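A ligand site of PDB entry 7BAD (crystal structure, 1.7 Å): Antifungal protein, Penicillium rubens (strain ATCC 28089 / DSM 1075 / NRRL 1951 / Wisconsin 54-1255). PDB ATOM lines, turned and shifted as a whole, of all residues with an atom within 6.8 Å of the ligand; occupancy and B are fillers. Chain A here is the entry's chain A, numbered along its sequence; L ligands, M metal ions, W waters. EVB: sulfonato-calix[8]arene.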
ATOM      1  N   LEU A   1      -0.647 -19.889  10.775  1.00  0.00           N
ATOM      2  CA  LEU A   1       0.192 -20.862  10.076  1.00  0.00           C
ATOM      3  C   LEU A   1       1.516 -21.018  10.837  1.00  0.00           C
ATOM      4  O   LEU A   1       2.107 -20.010  11.232  1.00  0.00           O
ATOM      5  CB  LEU A   1       0.449 -20.361   8.668  1.00  0.00           C
ATOM      6  CG  LEU A   1       1.264 -21.268   7.767  1.00  0.00           C
ATOM      7  CD1 LEU A   1       0.455 -22.490   7.346  1.00  0.00           C
ATOM      8  CD2 LEU A   1       1.704 -20.517   6.523  1.00  0.00           C
ATOM      9  N   SER A   2       1.984 -22.253  11.071  1.00  0.00           N
ATOM     10  CA  SER A   2       3.253 -22.464  11.770  1.00  0.00           C
ATOM     11  C   SER A   2       4.279 -23.248  10.954  1.00  0.00           C
ATOM     12  O   SER A   2       5.344 -23.534  11.480  1.00  0.00           O
ATOM     13  CB  SER A   2       3.032 -23.106  13.137  1.00  0.00           C
ATOM     14  OG  SER A   2       2.469 -24.397  12.914  1.00  0.00           O
ATOM     15  N   LYS A   3       3.936 -23.669   9.707  1.00  0.00           N
ATOM     16  CA  LYS A   3       4.845 -24.339   8.750  1.00  0.00           C
ATOM     17  C   LYS A   3       4.944 -23.387   7.550  1.00  0.00           C
ATOM     18  O   LYS A   3       3.911 -23.003   6.986  1.00  0.00           O
ATOM     19  CB  LYS A   3       4.309 -25.688   8.283  1.00  0.00           C
ATOM     20  CG  LYS A   3       4.965 -26.855   8.989  1.00  0.00           C
ATOM     21  CD  LYS A   3       4.579 -28.186   8.352  1.00  0.00           C
ATOM     22  CE  LYS A   3       5.687 -28.733   7.500  1.00  0.00           C
ATOM     23  NZ  LYS A   3       5.306 -30.002   6.819  1.00  0.00           N
ATOM     24  N   PHE A   4       6.156 -23.007   7.163  1.00  0.00           N
ATOM     25  CA  PHE A   4       6.367 -22.011   6.101  1.00  0.00           C
ATOM     26  C   PHE A   4       7.156 -22.570   4.954  1.00  0.00           C
ATOM     27  O   PHE A   4       8.116 -23.280   5.164  1.00  0.00           O
ATOM     28  CB  PHE A   4       7.106 -20.799   6.680  1.00  0.00           C
ATOM     29  CG  PHE A   4       6.459 -20.212   7.915  1.00  0.00           C
ATOM     30  CD1 PHE A   4       5.245 -19.576   7.847  1.00  0.00           C
ATOM     31  CD2 PHE A   4       7.077 -20.326   9.155  1.00  0.00           C
ATOM     32  CE1 PHE A   4       4.661 -19.029   8.974  1.00  0.00           C
ATOM     33  CE2 PHE A   4       6.482 -19.792  10.295  1.00  0.00           C
ATOM     34  CZ  PHE A   4       5.267 -19.144  10.195  1.00  0.00           C
ATOM     35  N   TYR A  17      12.128 -18.338   3.626  1.00  0.00           N
ATOM     36  CA  TYR A  17      10.681 -18.590   3.596  1.00  0.00           C
ATOM     37  C   TYR A  17       9.870 -17.344   3.853  1.00  0.00           C
ATOM     38  O   TYR A  17      10.305 -16.420   4.516  1.00  0.00           O
ATOM     39  CB  TYR A  17      10.310 -19.648   4.682  1.00  0.00           C
ATOM     40  CG  TYR A  17      10.731 -19.256   6.077  1.00  0.00           C
ATOM     41  CD1 TYR A  17      12.019 -19.511   6.531  1.00  0.00           C
ATOM     42  CD2 TYR A  17       9.828 -18.699   6.973  1.00  0.00           C
ATOM     43  CE1 TYR A  17      12.417 -19.130   7.793  1.00  0.00           C
ATOM     44  CE2 TYR A  17      10.232 -18.288   8.234  1.00  0.00           C
ATOM     45  CZ  TYR A  17      11.514 -18.581   8.667  1.00  0.00           C
ATOM     46  OH  TYR A  17      11.948 -18.199   9.910  1.00  0.00           O
ATOM     47  N   LEU A  18       8.592 -17.373   3.411  1.00  0.00           N
ATOM     48  CA  LEU A  18       7.674 -16.279   3.656  1.00  0.00           C
ATOM     49  C   LEU A  18       6.899 -16.488   4.961  1.00  0.00           C
ATOM     50  O   LEU A  18       6.345 -17.570   5.172  1.00  0.00           O
ATOM     51  CB  LEU A  18       6.629 -16.230   2.511  1.00  0.00           C
ATOM     52  CG  LEU A  18       6.893 -15.320   1.323  1.00  0.00           C
ATOM     53  CD1 LEU A  18       5.626 -15.222   0.422  1.00  0.00           C
ATOM     54  CD2 LEU A  18       7.300 -13.915   1.764  1.00  0.00           C
ATOM     55  N   LYS A  19       6.896 -15.471   5.839  1.00  0.00           N
ATOM     56  CA  LYS A  19       6.106 -15.455   7.085  1.00  0.00           C
ATOM     57  C   LYS A  19       5.592 -14.033   7.255  1.00  0.00           C
ATOM     58  O   LYS A  19       6.391 -13.100   7.273  1.00  0.00           O
ATOM     59  CB  LYS A  19       6.948 -15.860   8.305  1.00  0.00           C
ATOM     60  CG  LYS A  19       6.241 -15.629   9.655  1.00  0.00           C
ATOM     61  CD  LYS A  19       7.168 -16.012  10.808  1.00  0.00           C
ATOM     62  CE  LYS A  19       6.519 -15.793  12.158  1.00  0.00           C
ATOM     63  NZ  LYS A  19       7.413 -16.176  13.305  1.00  0.00           N
ATOM     64  N   GLY A  20       4.272 -13.868   7.341  1.00  0.00           N
ATOM     65  CA  GLY A  20       3.697 -12.540   7.427  1.00  0.00           C
ATOM     66  C   GLY A  20       3.962 -11.706   6.180  1.00  0.00           C
ATOM     67  O   GLY A  20       4.063 -10.476   6.260  1.00  0.00           O
ATOM     68  N   GLY A  21       4.094 -12.377   5.040  1.00  0.00           N
ATOM     69  CA  GLY A  21       4.336 -11.753   3.746  1.00  0.00           C
ATOM     70  C   GLY A  21       5.745 -11.236   3.505  1.00  0.00           C
ATOM     71  O   GLY A  21       6.004 -10.621   2.479  1.00  0.00           O
ATOM     72  N   LYS A  22       6.685 -11.558   4.415  1.00  0.00           N
ATOM     73  CA  LYS A  22       8.081 -11.107   4.268  1.00  0.00           C
ATOM     74  C   LYS A  22       9.067 -12.263   4.361  1.00  0.00           C
ATOM     75  O   LYS A  22       8.784 -13.276   5.012  1.00  0.00           O
ATOM     76  CB  LYS A  22       8.395 -10.054   5.337  1.00  0.00           C
ATOM     77  CG  LYS A  22       7.641  -8.736   5.103  1.00  0.00           C
ATOM     78  CD  LYS A  22       7.859  -7.733   6.211  1.00  0.00           C
ATOM     79  CE  LYS A  22       9.049  -6.857   5.930  1.00  0.00           C
ATOM     80  NZ  LYS A  22       8.891  -5.516   6.567  1.00  0.00           N
ATOM     81  N   HIS A  24      12.161 -14.495   5.561  1.00  0.00           N
ATOM     82  CA  HIS A  24      12.886 -14.855   6.769  1.00  0.00           C
ATOM     83  C   HIS A  24      13.870 -15.953   6.422  1.00  0.00           C
ATOM     84  O   HIS A  24      13.693 -16.650   5.432  1.00  0.00           O
ATOM     85  CB  HIS A  24      11.944 -15.312   7.904  1.00  0.00           C
ATOM     86  CG  HIS A  24      10.968 -14.280   8.368  1.00  0.00           C
ATOM     87  ND1 HIS A  24       9.935 -13.823   7.547  1.00  0.00           N
ATOM     88  CD2 HIS A  24      10.856 -13.696   9.580  1.00  0.00           C
ATOM     89  CE1 HIS A  24       9.216 -13.025   8.307  1.00  0.00           C
ATOM     90  NE2 HIS A  24       9.748 -12.875   9.518  1.00  0.00           N
ATOM     91  N   TYR A  45      10.034 -24.760   6.660  1.00  0.00           N
ATOM     92  CA  TYR A  45      10.426 -24.521   8.036  1.00  0.00           C
ATOM     93  C   TYR A  45       9.188 -24.691   8.951  1.00  0.00           C
ATOM     94  O   TYR A  45       8.230 -23.944   8.822  1.00  0.00           O
ATOM     95  CB  TYR A  45      10.947 -23.109   8.231  1.00  0.00           C
ATOM     96  CG  TYR A  45      11.333 -22.824   9.667  1.00  0.00           C
ATOM     97  CD1 TYR A  45      12.058 -23.745  10.413  1.00  0.00           C
ATOM     98  CD2 TYR A  45      10.986 -21.631  10.271  1.00  0.00           C
ATOM     99  CE1 TYR A  45      12.421 -23.478  11.732  1.00  0.00           C
ATOM    100  CE2 TYR A  45      11.367 -21.334  11.570  1.00  0.00           C
ATOM    101  CZ  TYR A  45      12.069 -22.283  12.307  1.00  0.00           C
ATOM    102  OH  TYR A  45      12.394 -22.005  13.612  1.00  0.00           O
ATOM    103  N   GLU A  47       8.107 -23.947  12.298  1.00  0.00           N
ATOM    104  CA  GLU A  47       8.501 -23.101  13.425  1.00  0.00           C
ATOM    105  C   GLU A  47       8.011 -23.676  14.797  1.00  0.00           C
ATOM    106  O   GLU A  47       8.673 -23.501  15.836  1.00  0.00           O
ATOM    107  CB  GLU A  47       7.996 -21.680  13.193  1.00  0.00           C
ATOM    108  CG  GLU A  47       8.445 -20.702  14.238  1.00  0.00           C
ATOM    109  CD  GLU A  47       8.298 -19.268  13.777  1.00  0.00           C
ATOM    110  OE1 GLU A  47       9.335 -18.589  13.597  1.00  0.00           O
ATOM    111  OE2 GLU A  47       7.144 -18.843  13.593  1.00  0.00           O
ATOM    112  N   HIS A  48       6.882 -24.377  14.761  1.00  0.00           N
ATOM    113  CA  HIS A  48       6.344 -24.978  15.995  1.00  0.00           C
ATOM    114  C   HIS A  48       7.234 -26.070  16.570  1.00  0.00           C
ATOM    115  O   HIS A  48       7.433 -26.140  17.797  1.00  0.00           O
ATOM    116  CB  HIS A  48       4.949 -25.509  15.768  1.00  0.00           C
ATOM    117  CG  HIS A  48       4.266 -25.838  17.063  1.00  0.00           C
ATOM    118  ND1 HIS A  48       3.975 -24.858  17.982  1.00  0.00           N
ATOM    119  CD2 HIS A  48       3.853 -27.042  17.560  1.00  0.00           C
ATOM    120  CE1 HIS A  48       3.389 -25.475  19.008  1.00  0.00           C
ATOM    121  NE2 HIS A  48       3.301 -26.789  18.791  1.00  0.00           N
ATOM    122  N   LYS A  50      10.479 -26.466  15.382  1.00  0.00           N
ATOM    123  CA  LYS A  50      11.859 -26.033  15.160  1.00  0.00           C
ATOM    124  C   LYS A  50      12.597 -27.039  14.272  1.00  0.00           C
ATOM    125  O   LYS A  50      13.680 -27.502  14.628  1.00  0.00           O
ATOM    126  CB  LYS A  50      12.584 -25.743  16.487  1.00  0.00           C
ATOM    127  CG  LYS A  50      11.897 -24.694  17.327  1.00  0.00           C
ATOM    128  CD  LYS A  50      12.347 -24.700  18.783  1.00  0.00           C
ATOM    129  CE  LYS A  50      11.466 -23.873  19.705  1.00  0.00           C
ATOM    130  NZ  LYS A  50      10.086 -23.730  19.174  1.00  0.00           N
HETATM  131  C11 EVB L   1       8.580 -10.840  16.742  1.00  0.00           C
HETATM  132  C12 EVB L   1       8.497 -11.785  15.739  1.00  0.00           C
HETATM  133  C13 EVB L   1       9.040 -11.524  14.507  1.00  0.00           C
HETATM  134  C14 EVB L   1       7.730 -13.088  16.008  1.00  0.00           C
HETATM  135  C15 EVB L   1       6.322 -10.394   9.507  1.00  0.00           C
HETATM  136  C17 EVB L   1       3.937  -9.798  10.014  1.00  0.00           C
HETATM  137  C18 EVB L   1       2.734 -10.009  10.679  1.00  0.00           C
HETATM  138  C19 EVB L   1       2.640 -10.972  11.647  1.00  0.00           C
HETATM  139  C20 EVB L   1       3.700 -11.801  11.929  1.00  0.00           C
HETATM  140  C21 EVB L   1       4.886 -11.649  11.236  1.00  0.00           C
HETATM  141  C22 EVB L   1       8.610 -14.325  16.165  1.00  0.00           C
HETATM  142  C23 EVB L   1       7.968 -15.526  16.420  1.00  0.00           C
HETATM  143  C1  EVB L   1       9.098  -7.984  11.751  1.00  0.00           C
HETATM  144  C2  EVB L   1       9.140  -9.376  11.903  1.00  0.00           C
HETATM  145  C3  EVB L   1       8.272 -10.152  11.150  1.00  0.00           C
HETATM  146  C4  EVB L   1       7.306  -9.567  10.321  1.00  0.00           C
HETATM  147  C5  EVB L   1       7.285  -8.182  10.171  1.00  0.00           C
HETATM  148  C6  EVB L   1       8.157  -7.405  10.900  1.00  0.00           C
HETATM  149  C7  EVB L   1      10.210  -9.997  12.823  1.00  0.00           C
HETATM  150  C8  EVB L   1       9.653 -10.308  14.227  1.00  0.00           C
HETATM  151  C9  EVB L   1       9.773  -9.387  15.239  1.00  0.00           C
HETATM  152  C10 EVB L   1       9.252  -9.661  16.490  1.00  0.00           C
HETATM  153  C16 EVB L   1       5.033 -10.605  10.303  1.00  0.00           C
HETATM  154  C24 EVB L   1       8.690 -16.703  16.634  1.00  0.00           C
HETATM  155  C25 EVB L   1      10.063 -16.682  16.524  1.00  0.00           C
HETATM  156  C26 EVB L   1      10.701 -15.484  16.255  1.00  0.00           C
HETATM  157  C27 EVB L   1       9.991 -14.305  16.097  1.00  0.00           C
HETATM  158  C28 EVB L   1       8.019 -18.048  16.928  1.00  0.00           C
HETATM  159  C29 EVB L   1       3.506 -12.889  12.975  1.00  0.00           C
HETATM  160  C30 EVB L   1       7.709 -18.241  18.415  1.00  0.00           C
HETATM  161  C31 EVB L   1       6.474 -17.896  18.943  1.00  0.00           C
HETATM  162  C32 EVB L   1       6.146 -18.213  20.273  1.00  0.00           C
HETATM  163  C33 EVB L   1       7.131 -18.767  21.083  1.00  0.00           C
HETATM  164  C34 EVB L   1       8.351 -19.128  20.556  1.00  0.00           C
HETATM  165  C35 EVB L   1       8.642 -18.888  19.223  1.00  0.00           C
HETATM  166  C36 EVB L   1       3.171 -14.263  12.378  1.00  0.00           C
HETATM  167  C37 EVB L   1       2.619 -14.419  11.122  1.00  0.00           C
HETATM  168  C38 EVB L   1       2.250 -15.686  10.701  1.00  0.00           C
HETATM  169  C39 EVB L   1       2.434 -16.798  11.498  1.00  0.00           C
HETATM  170  C40 EVB L   1       2.978 -16.653  12.743  1.00  0.00           C
HETATM  171  C41 EVB L   1       3.294 -15.390  13.188  1.00  0.00           C
HETATM  172  C42 EVB L   1       4.818 -17.824  20.954  1.00  0.00           C
HETATM  173  C43 EVB L   1       3.199 -17.873  13.634  1.00  0.00           C
HETATM  174  C44 EVB L   1       3.579 -18.535  20.380  1.00  0.00           C
HETATM  175  C45 EVB L   1       2.720 -17.790  19.582  1.00  0.00           C
HETATM  176  C46 EVB L   1       1.589 -18.373  19.048  1.00  0.00           C
HETATM  177  C47 EVB L   1       1.247 -19.687  19.403  1.00  0.00           C
HETATM  178  C48 EVB L   1       2.053 -20.428  20.283  1.00  0.00           C
HETATM  179  C49 EVB L   1       3.220 -19.831  20.767  1.00  0.00           C
HETATM  180  C50 EVB L   1       1.995 -18.157  14.555  1.00  0.00           C
HETATM  181  C51 EVB L   1       1.044 -19.054  14.116  1.00  0.00           C
HETATM  182  C52 EVB L   1      -0.018 -19.411  14.927  1.00  0.00           C
HETATM  183  C53 EVB L   1      -0.139 -18.884  16.191  1.00  0.00           C
HETATM  184  C54 EVB L   1       0.835 -18.020  16.661  1.00  0.00           C
HETATM  185  C55 EVB L   1       1.904 -17.659  15.839  1.00  0.00           C
HETATM  186  O1  EVB L   1       3.137 -16.513  19.175  1.00  0.00           O
HETATM  187  O2  EVB L   1       5.547 -17.281  18.080  1.00  0.00           O
HETATM  188  O3  EVB L   1       6.572 -15.488  16.510  1.00  0.00           O
HETATM  189  O4  EVB L   1       8.914 -12.422  13.454  1.00  0.00           O
HETATM  190  O5  EVB L   1       8.331 -11.548  11.277  1.00  0.00           O
HETATM  191  O6  EVB L   1       5.963 -12.499  11.577  1.00  0.00           O
HETATM  192  O7  EVB L   1       3.858 -15.239  14.441  1.00  0.00           O
HETATM  193  O8  EVB L   1       2.868 -16.760  16.297  1.00  0.00           O
HETATM  194  S64 EVB L   1       1.592 -22.144  20.811  1.00  0.00           S
HETATM  195  S65 EVB L   1       9.564 -19.907  21.654  1.00  0.00           S
HETATM  196  S66 EVB L   1      12.489 -15.439  16.054  1.00  0.00           S
HETATM  197  S67 EVB L   1       9.401  -8.418  17.794  1.00  0.00           S
HETATM  198  S68 EVB L   1       8.089  -5.591  10.689  1.00  0.00           S
HETATM  199  S69 EVB L   1       1.270  -8.958  10.395  1.00  0.00           S
HETATM  200  S70 EVB L   1       1.541 -15.882   9.064  1.00  0.00           S
HETATM  201  S71 EVB L   1      -1.289 -20.528  14.283  1.00  0.00           S
HETATM  202  C72 EVB L   1       0.703 -17.521  18.100  1.00  0.00           C
HETATM  203  O9  EVB L   1       2.833 -22.833  21.671  1.00  0.00           O
HETATM  204  O10 EVB L   1       0.236 -22.088  21.751  1.00  0.00           O
HETATM  205  O11 EVB L   1       1.235 -23.069  19.494  1.00  0.00           O
HETATM  206  O12 EVB L   1      10.845 -20.510  20.814  1.00  0.00           O
HETATM  207  O13 EVB L   1      10.089 -18.741  22.713  1.00  0.00           O
HETATM  208  O14 EVB L   1       8.825 -21.134  22.493  1.00  0.00           O
HETATM  209  O15 EVB L   1      13.143 -16.811  16.683  1.00  0.00           O
HETATM  210  O16 EVB L   1      12.724 -15.308  14.459  1.00  0.00           O
HETATM  211  O17 EVB L   1      13.133 -14.208  16.913  1.00  0.00           O
HETATM  212  O18 EVB L   1       9.634  -9.065  19.299  1.00  0.00           O
HETATM  213  O19 EVB L   1       7.992  -7.563  17.701  1.00  0.00           O
HETATM  214  O20 EVB L   1      10.661  -7.470  17.372  1.00  0.00           O
HETATM  215  O21 EVB L   1       6.530  -5.086  10.518  1.00  0.00           O
HETATM  216  O22 EVB L   1       8.788  -4.959  12.026  1.00  0.00           O
HETATM  217  O23 EVB L   1       8.948  -5.361   9.317  1.00  0.00           O
HETATM  218  O24 EVB L   1       1.183  -8.050  11.758  1.00  0.00           O
HETATM  219  O25 EVB L   1      -0.028  -9.948  10.199  1.00  0.00           O
HETATM  220  O26 EVB L   1       1.498  -8.047   9.060  1.00  0.00           O
HETATM  221  O27 EVB L   1       0.519 -17.161   8.989  1.00  0.00           O
HETATM  222  O28 EVB L   1       2.758 -16.181   8.006  1.00  0.00           O
HETATM  223  O29 EVB L   1       0.723 -14.500   8.670  1.00  0.00           O
HETATM  224  O30 EVB L   1      -0.677 -21.706  13.333  1.00  0.00           O
HETATM  225  O31 EVB L   1      -2.117 -21.215  15.546  1.00  0.00           O
HETATM  226  O32 EVB L   1      -2.375 -19.666  13.385  1.00  0.00           O
HETATM  227 ZN    ZN M   1       2.614 -28.158  20.119  1.00  0.00          ZN
HETATM  228  O   HOH W   1       2.373 -17.277   5.627  1.00  0.00           O
HETATM  229  O   HOH W   2      10.153 -14.835  12.903  1.00  0.00           O
HETATM  230  O   HOH W   3       7.853  -5.314  14.530  1.00  0.00           O
HETATM  231  O   HOH W   4      13.813 -21.314  19.486  1.00  0.00           O
HETATM  232  O   HOH W   5      15.702 -17.537  17.702  1.00  0.00           O
HETATM  233  O   HOH W   6       4.742  -4.069   8.743  1.00  0.00           O
HETATM  234  O   HOH W   7      13.381 -17.705  13.339  1.00  0.00           O
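NE2 of His 24 is in hydrogen-bond range of O5 of the ligand, at 2.6 Å.
The side-chain amino group (NZ) of Lys 22 is in salt-bridge range of an oxygen (O23) of the ligand (2.8 Å).
The backbone NH (N) of Gly 20 lies within hydrogen-bond range of an oxygen (O28) of the ligand, at 2.8 Å.
O30 of the ligand is in hydrogen-bond range of N of Leu 1 (3.1 Å).
The side-chain amino group of Lys 19 sits close to an oxygen (O3) of the ligand, at 3.4 Å.
NZ of Lys 50 is in salt-bridge range of O12 of the ligand (3.7 Å).
A ring nitrogen (ND1) of His 24 is in hydrogen-bond range of the backbone carbonyl oxygen (O) of Lys 22, at 2.8 Å.
The backbone carbonyl oxygen (O) of Tyr 17 is in hydrogen-bond range of the backbone NH (N) of His 24.
The side-chain carboxylate of Glu 47 lies within salt-bridge range of the side-chain amino group of Lys 19.
The backbone NH of Glu 47 lies within hydrogen-bond range of the backbone carbonyl oxygen of Ser 2 (2.9 Å).
The backbone carbonyl oxygen (O) of Tyr 45 lies within hydrogen-bond range of the backbone NH (N) of Phe 4.
Residues that only touch the ligand: Ser 2 (3.5 Å), Phe 4 (3.6 Å), Glu 47 (3.4 Å) and His 48 (3.3 Å).
Hydrophobic or aromatic side chains that line the ligand: Leu 1, Phe 4, His 24 and His 48.
Of the 15 residues printed, 10 come within 4 Å of the ligand.
The nearest printed residue that does not touch the ligand is Leu 18 (4.8 Å).
Water W2 bridges an oxygen (O4) of the ligand (2.8 Å) and the side-chain amino group of Lys 19 (3.1 Å).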
